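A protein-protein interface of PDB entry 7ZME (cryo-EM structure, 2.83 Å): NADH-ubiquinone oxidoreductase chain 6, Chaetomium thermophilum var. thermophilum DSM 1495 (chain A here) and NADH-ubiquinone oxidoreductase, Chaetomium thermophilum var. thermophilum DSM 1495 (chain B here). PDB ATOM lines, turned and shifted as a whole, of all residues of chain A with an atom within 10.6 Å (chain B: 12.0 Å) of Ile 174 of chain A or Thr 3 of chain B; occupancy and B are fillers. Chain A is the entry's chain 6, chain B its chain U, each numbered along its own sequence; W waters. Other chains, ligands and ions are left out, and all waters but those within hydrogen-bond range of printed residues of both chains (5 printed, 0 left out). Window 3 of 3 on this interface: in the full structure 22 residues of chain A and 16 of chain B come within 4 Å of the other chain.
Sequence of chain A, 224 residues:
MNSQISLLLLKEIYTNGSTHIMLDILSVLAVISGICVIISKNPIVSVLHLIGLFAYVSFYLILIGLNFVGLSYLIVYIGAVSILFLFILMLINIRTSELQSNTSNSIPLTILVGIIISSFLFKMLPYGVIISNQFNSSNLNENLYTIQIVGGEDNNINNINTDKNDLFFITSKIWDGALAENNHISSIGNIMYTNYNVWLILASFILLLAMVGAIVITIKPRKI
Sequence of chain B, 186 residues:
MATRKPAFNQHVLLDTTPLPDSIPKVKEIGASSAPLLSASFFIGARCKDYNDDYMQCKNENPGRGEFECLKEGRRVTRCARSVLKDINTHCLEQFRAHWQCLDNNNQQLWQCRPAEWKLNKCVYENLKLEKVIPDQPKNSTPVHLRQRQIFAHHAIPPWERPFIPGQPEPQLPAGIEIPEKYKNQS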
ATOM      1  N   PHE A 169      36.799 -14.243  -6.000  1.00  0.00           N
ATOM      2  CA  PHE A 169      35.502 -14.573  -5.370  1.00  0.00           C
ATOM      3  C   PHE A 169      35.730 -14.953  -3.914  1.00  0.00           C
ATOM      4  O   PHE A 169      36.675 -15.683  -3.621  1.00  0.00           O
ATOM      5  CB  PHE A 169      34.792 -15.650  -6.186  1.00  0.00           C
ATOM      6  CG  PHE A 169      34.394 -15.221  -7.573  1.00  0.00           C
ATOM      7  CD1 PHE A 169      33.318 -14.376  -7.769  1.00  0.00           C
ATOM      8  CD2 PHE A 169      35.095 -15.665  -8.679  1.00  0.00           C
ATOM      9  CE1 PHE A 169      32.952 -13.987  -9.048  1.00  0.00           C
ATOM     10  CE2 PHE A 169      34.729 -15.271  -9.956  1.00  0.00           C
ATOM     11  CZ  PHE A 169      33.658 -14.431 -10.137  1.00  0.00           C
ATOM     12  N   ILE A 170      34.867 -14.464  -3.034  1.00  0.00           N
ATOM     13  CA  ILE A 170      35.013 -14.715  -1.571  1.00  0.00           C
ATOM     14  C   ILE A 170      33.779 -15.474  -1.073  1.00  0.00           C
ATOM     15  O   ILE A 170      32.662 -15.079  -1.431  1.00  0.00           O
ATOM     16  CB  ILE A 170      35.301 -13.404  -0.811  1.00  0.00           C
ATOM     17  CG1 ILE A 170      35.840 -13.662   0.597  1.00  0.00           C
ATOM     18  CG2 ILE A 170      34.111 -12.462  -0.806  1.00  0.00           C
ATOM     19  CD1 ILE A 170      37.298 -14.025   0.631  1.00  0.00           C
ATOM     20  N   THR A 171      33.982 -16.567  -0.341  1.00  0.00           N
ATOM     21  CA  THR A 171      32.874 -17.320   0.227  1.00  0.00           C
ATOM     22  C   THR A 171      33.094 -17.525   1.717  1.00  0.00           C
ATOM     23  O   THR A 171      34.223 -17.689   2.183  1.00  0.00           O
ATOM     24  CB  THR A 171      32.678 -18.691  -0.444  1.00  0.00           C
ATOM     25  OG1 THR A 171      33.737 -19.574  -0.060  1.00  0.00           O
ATOM     26  CG2 THR A 171      32.645 -18.562  -1.953  1.00  0.00           C
ATOM     27  N   SER A 172      31.997 -17.550   2.479  1.00  0.00           N
ATOM     28  CA  SER A 172      32.057 -17.796   3.944  1.00  0.00           C
ATOM     29  C   SER A 172      31.047 -18.891   4.284  1.00  0.00           C
ATOM     30  O   SER A 172      30.554 -19.530   3.348  1.00  0.00           O
ATOM     31  CB  SER A 172      31.799 -16.550   4.729  1.00  0.00           C
ATOM     32  OG  SER A 172      30.440 -16.172   4.641  1.00  0.00           O
ATOM     33  N   LYS A 173      30.716 -19.067   5.564  1.00  0.00           N
ATOM     34  CA  LYS A 173      29.836 -20.197   5.960  1.00  0.00           C
ATOM     35  C   LYS A 173      28.529 -19.728   6.616  1.00  0.00           C
ATOM     36  O   LYS A 173      28.515 -18.607   7.133  1.00  0.00           O
ATOM     37  CB  LYS A 173      30.653 -21.094   6.888  1.00  0.00           C
ATOM     38  CG  LYS A 173      30.874 -20.592   8.306  1.00  0.00           C
ATOM     39  CD  LYS A 173      31.645 -21.572   9.153  1.00  0.00           C
ATOM     40  CE  LYS A 173      32.965 -21.980   8.537  1.00  0.00           C
ATOM     41  NZ  LYS A 173      33.681 -22.961   9.385  1.00  0.00           N
ATOM     42  N   ILE A 174      27.455 -20.529   6.544  1.00  0.00           N
ATOM     43  CA  ILE A 174      26.194 -20.215   7.295  1.00  0.00           C
ATOM     44  C   ILE A 174      25.747 -21.467   8.040  1.00  0.00           C
ATOM     45  O   ILE A 174      26.093 -22.566   7.609  1.00  0.00           O
ATOM     46  CB  ILE A 174      25.022 -19.639   6.466  1.00  0.00           C
ATOM     47  CG1 ILE A 174      24.697 -20.475   5.227  1.00  0.00           C
ATOM     48  CG2 ILE A 174      25.232 -18.167   6.144  1.00  0.00           C
ATOM     49  CD1 ILE A 174      23.373 -20.116   4.599  1.00  0.00           C
ATOM     50  N   TRP A 175      25.027 -21.280   9.136  1.00  0.00           N
ATOM     51  CA  TRP A 175      24.587 -22.422   9.969  1.00  0.00           C
ATOM     52  C   TRP A 175      23.095 -22.714   9.782  1.00  0.00           C
ATOM     53  O   TRP A 175      22.741 -23.896   9.748  1.00  0.00           O
ATOM     54  CB  TRP A 175      24.983 -22.129  11.417  1.00  0.00           C
ATOM     55  CG  TRP A 175      26.469 -22.050  11.566  1.00  0.00           C
ATOM     56  CD1 TRP A 175      27.227 -20.922  11.660  1.00  0.00           C
ATOM     57  CD2 TRP A 175      27.391 -23.153  11.577  1.00  0.00           C
ATOM     58  NE1 TRP A 175      28.551 -21.247  11.761  1.00  0.00           N
ATOM     59  CE2 TRP A 175      28.684 -22.608  11.710  1.00  0.00           C
ATOM     60  CE3 TRP A 175      27.251 -24.543  11.504  1.00  0.00           C
ATOM     61  CZ2 TRP A 175      29.824 -23.405  11.771  1.00  0.00           C
ATOM     62  CZ3 TRP A 175      28.378 -25.331  11.564  1.00  0.00           C
ATOM     63  CH2 TRP A 175      29.645 -24.765  11.699  1.00  0.00           C
ATOM     64  N   ASP A 176      22.268 -21.678   9.661  1.00  0.00           N
ATOM     65  CA  ASP A 176      20.804 -21.839   9.450  1.00  0.00           C
ATOM     66  C   ASP A 176      20.508 -22.490   8.090  1.00  0.00           C
ATOM     67  O   ASP A 176      19.597 -23.329   8.023  1.00  0.00           O
ATOM     68  CB  ASP A 176      20.049 -20.541   9.741  1.00  0.00           C
ATOM     69  CG  ASP A 176      20.754 -19.283   9.264  1.00  0.00           C
ATOM     70  OD1 ASP A 176      20.341 -18.187   9.690  1.00  0.00           O
ATOM     71  OD2 ASP A 176      21.696 -19.399   8.458  1.00  0.00           O
ATOM     72  N   GLY A 177      21.246 -22.118   7.051  1.00  0.00           N
ATOM     73  CA  GLY A 177      21.044 -22.688   5.707  1.00  0.00           C
ATOM     74  C   GLY A 177      21.799 -23.979   5.511  1.00  0.00           C
ATOM     75  O   GLY A 177      21.659 -24.570   4.439  1.00  0.00           O
ATOM     76  N   ALA A 178      22.592 -24.391   6.496  1.00  0.00           N
ATOM     77  CA  ALA A 178      23.311 -25.681   6.419  1.00  0.00           C
ATOM     78  C   ALA A 178      22.697 -26.729   7.347  1.00  0.00           C
ATOM     79  O   ALA A 178      23.393 -27.718   7.609  1.00  0.00           O
ATOM     80  CB  ALA A 178      24.768 -25.486   6.734  1.00  0.00           C
ATOM     81  N   LEU A 179      21.478 -26.528   7.853  1.00  0.00           N
ATOM     82  CA  LEU A 179      20.972 -27.512   8.845  1.00  0.00           C
ATOM     83  C   LEU A 179      20.855 -28.904   8.217  1.00  0.00           C
ATOM     84  O   LEU A 179      21.410 -29.846   8.790  1.00  0.00           O
ATOM     85  CB  LEU A 179      19.608 -27.041   9.356  1.00  0.00           C
ATOM     86  CG  LEU A 179      18.837 -28.051  10.205  1.00  0.00           C
ATOM     87  CD1 LEU A 179      19.420 -28.154  11.603  1.00  0.00           C
ATOM     88  CD2 LEU A 179      17.368 -27.688  10.278  1.00  0.00           C
ATOM     89  N   ALA A 180      20.197 -29.023   7.068  1.00  0.00           N
ATOM     90  CA  ALA A 180      20.106 -30.315   6.354  1.00  0.00           C
ATOM     91  C   ALA A 180      20.380 -30.092   4.868  1.00  0.00           C
ATOM     92  O   ALA A 180      19.426 -30.192   4.100  1.00  0.00           O
ATOM     93  CB  ALA A 180      18.740 -30.890   6.568  1.00  0.00           C
ATOM     94  N   GLU A 181      21.760 -29.909   4.550  1.00  0.00           N
ATOM     95  CA  GLU A 181      22.087 -29.668   3.118  1.00  0.00           C
ATOM     96  C   GLU A 181      21.603 -30.826   2.255  1.00  0.00           C
ATOM     97  O   GLU A 181      21.806 -31.981   2.656  1.00  0.00           O
ATOM     98  CB  GLU A 181      23.562 -29.360   2.880  1.00  0.00           C
ATOM     99  CG  GLU A 181      23.969 -29.269   1.427  1.00  0.00           C
ATOM    100  CD  GLU A 181      25.280 -29.985   1.160  1.00  0.00           C
ATOM    101  OE1 GLU A 181      25.824 -30.573   2.112  1.00  0.00           O
ATOM    102  OE2 GLU A 181      25.745 -29.960   0.006  1.00  0.00           O
ATOM    103  N   HIS A 184      22.153 -31.891  -5.055  1.00  0.00           N
ATOM    104  CA  HIS A 184      21.432 -31.152  -6.118  1.00  0.00           C
ATOM    105  C   HIS A 184      20.265 -31.985  -6.653  1.00  0.00           C
ATOM    106  O   HIS A 184      19.221 -31.399  -6.937  1.00  0.00           O
ATOM    107  CB  HIS A 184      22.410 -30.759  -7.224  1.00  0.00           C
ATOM    108  CG  HIS A 184      23.362 -29.672  -6.862  1.00  0.00           C
ATOM    109  ND1 HIS A 184      24.229 -29.123  -7.781  1.00  0.00           N
ATOM    110  CD2 HIS A 184      23.590 -29.031  -5.699  1.00  0.00           C
ATOM    111  CE1 HIS A 184      24.950 -28.192  -7.201  1.00  0.00           C
ATOM    112  NE2 HIS A 184      24.578 -28.116  -5.923  1.00  0.00           N
ATOM    113  N   MET B   1      30.833 -13.068   3.258  1.00  0.00           N
ATOM    114  CA  MET B   1      31.116 -13.657   1.960  1.00  0.00           C
ATOM    115  C   MET B   1      30.048 -14.683   1.600  1.00  0.00           C
ATOM    116  O   MET B   1      29.328 -15.161   2.471  1.00  0.00           O
ATOM    117  CB  MET B   1      32.505 -14.280   1.966  1.00  0.00           C
ATOM    118  N   ALA B   2      29.848 -14.911   0.299  1.00  0.00           N
ATOM    119  CA  ALA B   2      28.873 -15.903  -0.219  1.00  0.00           C
ATOM    120  C   ALA B   2      28.726 -17.249   0.486  1.00  0.00           C
ATOM    121  O   ALA B   2      29.710 -17.793   0.994  1.00  0.00           O
ATOM    122  CB  ALA B   2      29.095 -16.082  -1.689  1.00  0.00           C
ATOM    123  N   THR B   3      27.496 -17.771   0.457  1.00  0.00           N
ATOM    124  CA  THR B   3      27.178 -19.047   1.138  1.00  0.00           C
ATOM    125  C   THR B   3      27.360 -20.203   0.154  1.00  0.00           C
ATOM    126  O   THR B   3      27.071 -21.350   0.534  1.00  0.00           O
ATOM    127  CB  THR B   3      25.754 -18.982   1.690  1.00  0.00           C
ATOM    128  OG1 THR B   3      24.867 -19.123   0.581  1.00  0.00           O
ATOM    129  CG2 THR B   3      25.463 -17.686   2.410  1.00  0.00           C
ATOM    130  N   ARG B   4      27.821 -19.901  -1.059  1.00  0.00           N
ATOM    131  CA  ARG B   4      28.075 -20.956  -2.061  1.00  0.00           C
ATOM    132  C   ARG B   4      29.278 -21.777  -1.611  1.00  0.00           C
ATOM    133  O   ARG B   4      30.223 -21.193  -1.063  1.00  0.00           O
ATOM    134  CB  ARG B   4      28.255 -20.365  -3.460  1.00  0.00           C
ATOM    135  CG  ARG B   4      29.385 -19.359  -3.600  1.00  0.00           C
ATOM    136  CD  ARG B   4      29.797 -19.261  -5.053  1.00  0.00           C
ATOM    137  NE  ARG B   4      31.081 -18.599  -5.203  1.00  0.00           N
ATOM    138  CZ  ARG B   4      32.255 -19.219  -5.173  1.00  0.00           C
ATOM    139  NH1 ARG B   4      33.372 -18.531  -5.324  1.00  0.00           N
ATOM    140  NH2 ARG B   4      32.309 -20.525  -4.988  1.00  0.00           N
ATOM    141  N   LYS B   5      29.223 -23.092  -1.837  1.00  0.00           N
ATOM    142  CA  LYS B   5      30.359 -23.967  -1.474  1.00  0.00           C
ATOM    143  C   LYS B   5      31.428 -23.842  -2.562  1.00  0.00           C
ATOM    144  O   LYS B   5      31.114 -24.108  -3.731  1.00  0.00           O
ATOM    145  CB  LYS B   5      29.863 -25.402  -1.320  1.00  0.00           C
ATOM    146  CG  LYS B   5      28.695 -25.584  -0.359  1.00  0.00           C
ATOM    147  CD  LYS B   5      28.255 -27.027  -0.226  1.00  0.00           C
ATOM    148  CE  LYS B   5      27.858 -27.650  -1.547  1.00  0.00           C
ATOM    149  NZ  LYS B   5      26.692 -26.962  -2.147  1.00  0.00           N
ATOM    150  N   PRO B   6      32.675 -23.452  -2.219  1.00  0.00           N
ATOM    151  CA  PRO B   6      33.729 -23.255  -3.212  1.00  0.00           C
ATOM    152  C   PRO B   6      34.163 -24.528  -3.952  1.00  0.00           C
ATOM    153  O   PRO B   6      34.198 -25.574  -3.336  1.00  0.00           O
ATOM    154  CB  PRO B   6      34.891 -22.739  -2.354  1.00  0.00           C
ATOM    155  CG  PRO B   6      34.616 -23.262  -0.970  1.00  0.00           C
ATOM    156  CD  PRO B   6      33.114 -23.171  -0.852  1.00  0.00           C
ATOM    157  N   ALA B   7      34.484 -24.414  -5.241  1.00  0.00           N
ATOM    158  CA  ALA B   7      34.978 -25.561  -5.984  1.00  0.00           C
ATOM    159  C   ALA B   7      36.436 -25.441  -6.382  1.00  0.00           C
ATOM    160  O   ALA B   7      37.043 -26.446  -6.750  1.00  0.00           O
ATOM    161  CB  ALA B   7      34.136 -25.786  -7.250  1.00  0.00           C
ATOM    162  N   ASN B   9      38.802 -23.196  -4.456  1.00  0.00           N
ATOM    163  CA  ASN B   9      39.456 -22.368  -3.453  1.00  0.00           C
ATOM    164  C   ASN B   9      40.868 -22.877  -3.192  1.00  0.00           C
ATOM    165  O   ASN B   9      41.075 -24.072  -2.962  1.00  0.00           O
ATOM    166  CB  ASN B   9      38.644 -22.364  -2.162  1.00  0.00           C
ATOM    167  CG  ASN B   9      38.307 -23.760  -1.685  1.00  0.00           C
ATOM    168  OD1 ASN B   9      37.758 -24.567  -2.431  1.00  0.00           O
ATOM    169  ND2 ASN B   9      38.634 -24.053  -0.437  1.00  0.00           N
ATOM    170  N   TYR B  54      16.751 -14.842  19.586  1.00  0.00           N
ATOM    171  CA  TYR B  54      17.694 -14.259  18.600  1.00  0.00           C
ATOM    172  C   TYR B  54      17.189 -14.547  17.181  1.00  0.00           C
ATOM    173  O   TYR B  54      17.371 -13.685  16.307  1.00  0.00           O
ATOM    174  CB  TYR B  54      19.081 -14.862  18.830  1.00  0.00           C
ATOM    175  CG  TYR B  54      20.113 -14.610  17.762  1.00  0.00           C
ATOM    176  CD1 TYR B  54      20.608 -13.338  17.535  1.00  0.00           C
ATOM    177  CD2 TYR B  54      20.610 -15.647  16.992  1.00  0.00           C
ATOM    178  CE1 TYR B  54      21.563 -13.098  16.563  1.00  0.00           C
ATOM    179  CE2 TYR B  54      21.564 -15.426  16.015  1.00  0.00           C
ATOM    180  CZ  TYR B  54      22.045 -14.147  15.804  1.00  0.00           C
ATOM    181  OH  TYR B  54      22.984 -13.909  14.846  1.00  0.00           O
ATOM    182  N   MET B  55      16.558 -15.697  16.967  1.00  0.00           N
ATOM    183  CA  MET B  55      16.048 -16.108  15.630  1.00  0.00           C
ATOM    184  C   MET B  55      14.817 -15.295  15.234  1.00  0.00           C
ATOM    185  O   MET B  55      14.668 -15.017  14.039  1.00  0.00           O
ATOM    186  CB  MET B  55      15.770 -17.614  15.602  1.00  0.00           C
ATOM    187  CG  MET B  55      17.004 -18.455  15.843  1.00  0.00           C
ATOM    188  SD  MET B  55      18.271 -18.253  14.575  1.00  0.00           S
ATOM    189  CE  MET B  55      17.582 -19.238  13.247  1.00  0.00           C
ATOM    190  N   LYS B  58      15.987 -11.771  14.183  1.00  0.00           N
ATOM    191  CA  LYS B  58      16.477 -11.688  12.813  1.00  0.00           C
ATOM    192  C   LYS B  58      15.331 -11.724  11.815  1.00  0.00           C
ATOM    193  O   LYS B  58      15.362 -11.016  10.803  1.00  0.00           O
ATOM    194  CB  LYS B  58      17.473 -12.811  12.545  1.00  0.00           C
ATOM    195  CG  LYS B  58      18.800 -12.610  13.240  1.00  0.00           C
ATOM    196  CD  LYS B  58      19.712 -13.792  13.042  1.00  0.00           C
ATOM    197  CE  LYS B  58      20.625 -13.584  11.855  1.00  0.00           C
ATOM    198  NZ  LYS B  58      21.702 -14.607  11.831  1.00  0.00           N
ATOM    199  N   GLY B  65      19.151  -8.142   9.966  1.00  0.00           N
ATOM    200  CA  GLY B  65      19.237  -8.660  11.320  1.00  0.00           C
ATOM    201  C   GLY B  65      20.631  -9.023  11.779  1.00  0.00           C
ATOM    202  O   GLY B  65      20.823  -9.244  12.979  1.00  0.00           O
ATOM    203  N   GLU B  66      21.592  -9.161  10.865  1.00  0.00           N
ATOM    204  CA  GLU B  66      22.992  -9.420  11.302  1.00  0.00           C
ATOM    205  C   GLU B  66      23.416  -8.242  12.167  1.00  0.00           C
ATOM    206  O   GLU B  66      23.805  -8.469  13.324  1.00  0.00           O
ATOM    207  CB  GLU B  66      23.936  -9.525  10.102  1.00  0.00           C
ATOM    208  CG  GLU B  66      23.700 -10.746   9.232  1.00  0.00           C
ATOM    209  CD  GLU B  66      22.490 -10.688   8.312  1.00  0.00           C
ATOM    210  OE1 GLU B  66      22.064  -9.570   7.959  1.00  0.00           O
ATOM    211  OE2 GLU B  66      21.971 -11.764   7.960  1.00  0.00           O
HETATM  212  O   HOH W   1      30.388 -21.853   1.694  1.00  0.00           O
HETATM  213  O   HOH W   2      23.916 -29.022  -2.463  1.00  0.00           O
HETATM  214  O   HOH W   3      31.243 -15.564  -4.234  1.00  0.00           O
HETATM  215  O   HOH W   4      27.773 -16.611   4.647  1.00  0.00           O
HETATM  216  O   HOH W   5      25.466 -25.564  -4.413  1.00  0.00           O
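OG of Ser 172 of chain A is in hydrogen-bond range of O of Met 1 of chain B.
The backbone carbonyl oxygen of Ile 170 of chain A sits at hydrogen-bond distance from the backbone NH of Ala 2 of chain B.
The backbone NH (N) of Ser 172 of chain A lies within hydrogen-bond range of the backbone carbonyl oxygen (O) of Ala 2 of chain B.
NZ of Lys 5 of chain B lies within salt-bridge range of OE2 of Glu 181 of chain A (3.8 Å).
Ile 174 of chain A touches one residue of chain B.
Thr 3 of chain B touches one residue of chain A.
Ser 172 of chain A touches just these residues of chain B: Met 1 and Ala 2.
No residue of chain B comes within 4 Å of Lys 173 of chain A.
No residue of chain B comes within 4 Å of Asp 176 of chain A.
No residue of chain B comes within 4 Å of Gly 177 of chain A.
No residue of chain B comes within 4 Å of Ala 178 of chain A.
Of chain A, only Ile 170, Thr 171 and Ser 172 come within 4 Å of Met 1 of chain B.
Of chain A, only Ile 170 (3.3 Å), Thr 171 (3.3 Å) and Ser 172 (2.7 Å) come within 4 Å of Ala 2 of chain B.
Printed residues of chain B within 4 Å of Phe 169 of chain A: Arg 4.
Printed residues of chain A within 4 Å of Lys 5 of chain B: Glu 181 (3.5 Å).
Of the printed residues of chain B, Ile 170 of chain A touches Met 1 and Ala 2.
Of the printed residues of chain A, Arg 4 of chain B touches Phe 169 (3.3 Å) and Thr 171 (3.3 Å).
The nearest residue of chain A that does not touch Thr 3 of chain B is Ser 172 of chain A (4.1 Å).
Among the printed residues, pairs that only touch across the chains: Phe 169 of chain A with Arg 4 of chain B, Ile 170 of chain A with Met 1 of chain B, Thr 171 of chain A with Met 1 of chain B, Thr 171 of chain A with Ala 2 of chain B, Thr 171 of chain A with Arg 4 of chain B, Thr 171 of chain A with Pro 6 of chain B and Ile 174 of chain A with Thr 3 of chain B.
Water W4 lies within hydrogen-bond range of the side-chain hydroxyl (OG) of Ser 172 of chain A (2.7 Å), the backbone carbonyl oxygen (O) of Met 1 of chain B (3.0 Å) and the backbone carbonyl oxygen (O) of Lys 173 of chain A (3.3 Å).
Water W1 bridges O of Arg 4 of chain B (2.8 Å) and O of Ser 172 of chain A (2.9 Å).
Water W5 lies within hydrogen-bond range of NZ of Lys 5 of chain B (2.9 Å) and NE2 of His 184 of chain A (3.1 Å).
Water W3 lies within hydrogen-bond range of the backbone carbonyl oxygen of Ile 170 of chain A (3.2 Å) and the guanidinium group of Arg 4 of chain B (3.2 Å).
Water W2 bridges the side-chain carboxylate of Glu 181 of chain A (3.2 Å) and the side-chain amino group of Lys 5 of chain B (3.5 Å).
Of the 14 printed residues of chain A, 6 touch a printed residue of chain B.
Along chain A the printed residues that touch a printed residue of chain B span positions 169 to 181.
Printed residues of chain B that touch a printed residue of chain A: Met 1, Ala 2, Thr 3, Arg 4, Lys 5 and Pro 6.
Among the printed residues, 11 pairs touch across the chains.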
